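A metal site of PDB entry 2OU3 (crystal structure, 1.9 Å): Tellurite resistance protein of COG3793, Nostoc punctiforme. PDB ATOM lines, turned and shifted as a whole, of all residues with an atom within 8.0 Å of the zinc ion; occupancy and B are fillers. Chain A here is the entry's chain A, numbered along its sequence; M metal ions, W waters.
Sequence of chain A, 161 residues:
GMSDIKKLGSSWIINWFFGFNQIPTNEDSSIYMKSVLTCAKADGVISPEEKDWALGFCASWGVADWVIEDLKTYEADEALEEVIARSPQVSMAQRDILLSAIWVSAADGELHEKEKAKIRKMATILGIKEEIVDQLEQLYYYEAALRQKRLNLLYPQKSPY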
ATOM      1  N   ALA A  40      26.812   2.733  33.223  1.00  0.00           N
ATOM      2  CA  ALA A  40      27.636   3.156  32.093  1.00  0.00           C
ATOM      3  C   ALA A  40      29.000   3.660  32.583  1.00  0.00           C
ATOM      4  O   ALA A  40      30.035   3.316  32.017  1.00  0.00           O
ATOM      5  CB  ALA A  40      26.950   4.228  31.289  1.00  0.00           C
ATOM      6  N   VAL A  45      34.856   6.645  33.702  1.00  0.00           N
ATOM      7  CA  VAL A  45      34.128   7.875  33.476  1.00  0.00           C
ATOM      8  C   VAL A  45      33.049   7.662  32.409  1.00  0.00           C
ATOM      9  O   VAL A  45      32.942   6.625  31.741  1.00  0.00           O
ATOM     10  CB  VAL A  45      35.063   8.992  33.007  1.00  0.00           C
ATOM     11  N   ILE A  46      32.233   8.697  32.277  1.00  0.00           N
ATOM     12  CA  ILE A  46      31.206   8.747  31.264  1.00  0.00           C
ATOM     13  C   ILE A  46      31.497  10.056  30.525  1.00  0.00           C
ATOM     14  O   ILE A  46      31.692  11.086  31.144  1.00  0.00           O
ATOM     15  CB  ILE A  46      29.803   8.684  31.918  1.00  0.00           C
ATOM     16  CG1 ILE A  46      28.689   8.859  30.889  1.00  0.00           C
ATOM     17  CG2 ILE A  46      29.653   9.713  33.050  1.00  0.00           C
ATOM     18  CD1 ILE A  46      27.319   8.537  31.479  1.00  0.00           C
ATOM     19  N   SER A  47      31.600   9.990  29.204  1.00  0.00           N
ATOM     20  CA  SER A  47      31.869  11.195  28.415  1.00  0.00           C
ATOM     21  C   SER A  47      30.639  12.106  28.310  1.00  0.00           C
ATOM     22  O   SER A  47      29.498  11.655  28.498  1.00  0.00           O
ATOM     23  CB  SER A  47      32.306  10.829  27.015  1.00  0.00           C
ATOM     24  OG  SER A  47      31.247  10.185  26.330  1.00  0.00           O
ATOM     25  N   GLU A  49      29.345  13.265  25.633  1.00  0.00           N
ATOM     26  CA  GLU A  49      28.480  12.732  24.599  1.00  0.00           C
ATOM     27  C   GLU A  49      27.614  11.584  25.104  1.00  0.00           C
ATOM     28  O   GLU A  49      26.425  11.492  24.729  1.00  0.00           O
ATOM     29  CB  GLU A  49      29.297  12.251  23.391  1.00  0.00           C
ATOM     30  CG  GLU A  49      28.368  11.761  22.267  1.00  0.00           C
ATOM     31  CD  GLU A  49      29.082  11.488  20.939  1.00  0.00           C
ATOM     32  OE1 GLU A  49      30.324  11.380  20.930  1.00  0.00           O
ATOM     33  OE2 GLU A  49      28.396  11.402  19.909  1.00  0.00           O
ATOM     34  N   GLU A  50      28.187  10.698  25.895  1.00  0.00           N
ATOM     35  CA  GLU A  50      27.449   9.585  26.468  1.00  0.00           C
ATOM     36  C   GLU A  50      26.384  10.145  27.386  1.00  0.00           C
ATOM     37  O   GLU A  50      25.215   9.748  27.332  1.00  0.00           O
ATOM     38  CB  GLU A  50      28.370   8.648  27.249  1.00  0.00           C
ATOM     39  CG  GLU A  50      29.218   7.709  26.394  1.00  0.00           C
ATOM     40  CD  GLU A  50      30.304   7.026  27.199  1.00  0.00           C
ATOM     41  OE1 GLU A  50      30.757   7.604  28.209  1.00  0.00           O
ATOM     42  OE2 GLU A  50      30.702   5.920  26.831  1.00  0.00           O
ATOM     43  N   ALA A 101      22.407   1.110  29.530  1.00  0.00           N
ATOM     44  CA  ALA A 101      23.816   1.420  29.802  1.00  0.00           C
ATOM     45  C   ALA A 101      24.724   1.083  28.624  1.00  0.00           C
ATOM     46  O   ALA A 101      25.640   1.843  28.273  1.00  0.00           O
ATOM     47  CB  ALA A 101      24.303   0.661  31.052  1.00  0.00           C
ATOM     48  N   ILE A 102      24.441  -0.050  27.973  1.00  0.00           N
ATOM     49  CA  ILE A 102      25.162  -0.435  26.747  1.00  0.00           C
ATOM     50  C   ILE A 102      24.972   0.605  25.662  1.00  0.00           C
ATOM     51  O   ILE A 102      25.935   1.038  25.047  1.00  0.00           O
ATOM     52  CB  ILE A 102      24.683  -1.812  26.237  1.00  0.00           C
ATOM     53  CG1 ILE A 102      25.138  -2.893  27.221  1.00  0.00           C
ATOM     54  CG2 ILE A 102      25.219  -2.109  24.790  1.00  0.00           C
ATOM     55  CD1 ILE A 102      24.376  -4.247  27.106  1.00  0.00           C
ATOM     56  N   TRP A 103      23.715   1.011  25.426  1.00  0.00           N
ATOM     57  CA  TRP A 103      23.394   2.029  24.410  1.00  0.00           C
ATOM     58  C   TRP A 103      24.060   3.367  24.748  1.00  0.00           C
ATOM     59  O   TRP A 103      24.597   4.016  23.867  1.00  0.00           O
ATOM     60  CB  TRP A 103      21.900   2.234  24.278  1.00  0.00           C
ATOM     61  CG  TRP A 103      21.251   1.377  23.286  1.00  0.00           C
ATOM     62  CD1 TRP A 103      20.617   0.200  23.509  1.00  0.00           C
ATOM     63  CD2 TRP A 103      21.196   1.624  21.879  1.00  0.00           C
ATOM     64  NE1 TRP A 103      20.116  -0.302  22.307  1.00  0.00           N
ATOM     65  CE2 TRP A 103      20.479   0.545  21.296  1.00  0.00           C
ATOM     66  CE3 TRP A 103      21.690   2.631  21.058  1.00  0.00           C
ATOM     67  CZ2 TRP A 103      20.242   0.482  19.946  1.00  0.00           C
ATOM     68  CZ3 TRP A 103      21.445   2.564  19.708  1.00  0.00           C
ATOM     69  CH2 TRP A 103      20.746   1.495  19.160  1.00  0.00           C
ATOM     70  N   VAL A 104      24.026   3.753  26.023  1.00  0.00           N
ATOM     71  CA  VAL A 104      24.724   4.967  26.439  1.00  0.00           C
ATOM     72  C   VAL A 104      26.238   4.896  26.151  1.00  0.00           C
ATOM     73  O   VAL A 104      26.804   5.857  25.668  1.00  0.00           O
ATOM     74  CB  VAL A 104      24.499   5.252  27.929  1.00  0.00           C
ATOM     75  CG1 VAL A 104      25.441   6.361  28.414  1.00  0.00           C
ATOM     76  CG2 VAL A 104      23.015   5.660  28.179  1.00  0.00           C
ATOM     77  N   SER A 105      26.852   3.786  26.490  1.00  0.00           N
ATOM     78  CA  SER A 105      28.273   3.581  26.294  1.00  0.00           C
ATOM     79  C   SER A 105      28.609   3.622  24.796  1.00  0.00           C
ATOM     80  O   SER A 105      29.671   4.039  24.391  1.00  0.00           O
ATOM     81  CB  SER A 105      28.672   2.253  26.919  1.00  0.00           C
ATOM     82  OG  SER A 105      28.591   2.298  28.328  1.00  0.00           O
ATOM     83  N   ALA A 106      27.701   3.125  23.976  1.00  0.00           N
ATOM     84  CA  ALA A 106      27.911   3.108  22.527  1.00  0.00           C
ATOM     85  C   ALA A 106      27.762   4.485  21.887  1.00  0.00           C
ATOM     86  O   ALA A 106      28.146   4.663  20.740  1.00  0.00           O
ATOM     87  CB  ALA A 106      26.894   2.139  21.869  1.00  0.00           C
ATOM     88  N   ALA A 107      27.205   5.475  22.615  1.00  0.00           N
ATOM     89  CA  ALA A 107      26.792   6.761  22.028  1.00  0.00           C
ATOM     90  C   ALA A 107      27.958   7.562  21.497  1.00  0.00           C
ATOM     91  O   ALA A 107      27.787   8.364  20.584  1.00  0.00           O
ATOM     92  CB  ALA A 107      26.004   7.621  23.070  1.00  0.00           C
ATOM     93  N   ASP A 108      29.124   7.365  22.097  1.00  0.00           N
ATOM     94  CA  ASP A 108      30.311   8.103  21.701  1.00  0.00           C
ATOM     95  C   ASP A 108      31.287   7.223  20.914  1.00  0.00           C
ATOM     96  O   ASP A 108      32.468   7.536  20.852  1.00  0.00           O
ATOM     97  CB  ASP A 108      31.006   8.714  22.935  1.00  0.00           C
ATOM     98  CG  ASP A 108      31.575   7.670  23.899  1.00  0.00           C
ATOM     99  OD1 ASP A 108      31.113   6.493  23.976  1.00  0.00           O
ATOM    100  OD2 ASP A 108      32.510   8.048  24.627  1.00  0.00           O
ATOM    101  N   GLY A 109      30.791   6.135  20.329  1.00  0.00           N
ATOM    102  CA  GLY A 109      31.616   5.226  19.530  1.00  0.00           C
ATOM    103  C   GLY A 109      31.445   3.768  19.908  1.00  0.00           C
ATOM    104  O   GLY A 109      30.990   3.447  20.998  1.00  0.00           O
ATOM    105  N   GLU A 110      31.832   2.885  19.000  1.00  0.00           N
ATOM    106  CA  GLU A 110      31.653   1.435  19.199  1.00  0.00           C
ATOM    107  C   GLU A 110      32.277   0.945  20.509  1.00  0.00           C
ATOM    108  O   GLU A 110      33.325   1.470  20.938  1.00  0.00           O
ATOM    109  CB  GLU A 110      32.216   0.656  18.001  1.00  0.00           C
ATOM    110  N   LEU A 111      31.648  -0.038  21.145  1.00  0.00           N
ATOM    111  CA  LEU A 111      32.099  -0.505  22.464  1.00  0.00           C
ATOM    112  C   LEU A 111      33.505  -1.097  22.438  1.00  0.00           C
ATOM    113  O   LEU A 111      33.778  -2.033  21.717  1.00  0.00           O
ATOM    114  CB  LEU A 111      31.135  -1.549  23.037  1.00  0.00           C
ATOM    115  CG  LEU A 111      29.664  -1.130  23.139  1.00  0.00           C
ATOM    116  CD1 LEU A 111      28.809  -2.314  23.507  1.00  0.00           C
ATOM    117  CD2 LEU A 111      29.544  -0.002  24.131  1.00  0.00           C
ATOM    118  N   HIS A 112      34.379  -0.547  23.271  1.00  0.00           N
ATOM    119  CA  HIS A 112      35.732  -1.029  23.432  1.00  0.00           C
ATOM    120  C   HIS A 112      35.736  -2.200  24.424  1.00  0.00           C
ATOM    121  O   HIS A 112      34.725  -2.442  25.083  1.00  0.00           O
ATOM    122  CB  HIS A 112      36.613   0.121  23.931  1.00  0.00           C
ATOM    123  CG  HIS A 112      36.297   1.456  23.310  1.00  0.00           C
ATOM    124  N   GLU A 115      34.823  -1.049  27.928  1.00  0.00           N
ATOM    125  CA  GLU A 115      33.394  -0.847  28.183  1.00  0.00           C
ATOM    126  C   GLU A 115      32.696  -2.209  28.303  1.00  0.00           C
ATOM    127  O   GLU A 115      31.794  -2.367  29.117  1.00  0.00           O
ATOM    128  CB  GLU A 115      32.750   0.033  27.095  1.00  0.00           C
ATOM    129  CG  GLU A 115      33.045   1.538  27.243  1.00  0.00           C
ATOM    130  CD  GLU A 115      32.566   2.331  26.044  1.00  0.00           C
ATOM    131  OE1 GLU A 115      32.872   1.929  24.912  1.00  0.00           O
ATOM    132  OE2 GLU A 115      31.886   3.372  26.228  1.00  0.00           O
ATOM    133  N   LYS A 118      33.551  -3.303  31.922  1.00  0.00           N
ATOM    134  CA  LYS A 118      32.668  -2.533  32.824  1.00  0.00           C
ATOM    135  C   LYS A 118      31.272  -3.105  32.920  1.00  0.00           C
ATOM    136  O   LYS A 118      30.716  -3.290  34.026  1.00  0.00           O
ATOM    137  CB  LYS A 118      32.530  -1.096  32.317  1.00  0.00           C
ATOM    138  CG  LYS A 118      33.816  -0.258  32.423  1.00  0.00           C
ATOM    139  CD  LYS A 118      33.592   1.282  32.373  1.00  0.00           C
ATOM    140  CE  LYS A 118      32.658   1.743  31.264  1.00  0.00           C
ATOM    141  NZ  LYS A 118      32.634   3.242  31.131  1.00  0.00           N
HETATM  142 ZN    ZN M   1      31.457   4.888  25.026  1.00  0.00          ZN
HETATM  143  O   HOH W   1      33.407   5.956  25.560  1.00  0.00           O
HETATM  144  O   HOH W   2      32.263   3.962  23.205  1.00  0.00           O
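OE1 of Glu 50 sits at hydrogen-bond distance from N of Ser 47 (2.7 Å).
The side-chain carboxylate (OD2) of Asp 108 sits at hydrogen-bond distance from the side-chain hydroxyl (OG) of Ser 47, at 3.0 Å.
The backbone NH of His 112 lies within hydrogen-bond range of the side-chain carboxylate of Glu 115, at 3.3 Å.
The backbone carbonyl oxygen (O) of Ala 101 sits at hydrogen-bond distance from the side-chain hydroxyl (OG) of Ser 105 (3.0 Å).
Of the 20 residues printed, 4 come within 4 Å of the zinc ion.
The nearest printed residue that does not touch the zinc ion is Ala 106 (4.3 Å).
The zinc ion is bound by OD1 of Asp 108, 1.9 Å away.
The side-chain carboxylate (OE2) of Glu 115 is bound to the zinc ion (2.0 Å).
The backbone carbonyl oxygen (O) of Ser 105 binds the zinc ion, at 2.1 Å.
The zinc ion is bound by water W2, at 2.2 Å.
OE2 of Glu 50 is bound to the zinc ion, at 2.2 Å.
The zinc ion is bound by water W1.
Water W2 lies within hydrogen-bond range of the backbone carbonyl oxygen of Gly 109 and the side-chain carboxylate of Glu 115.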
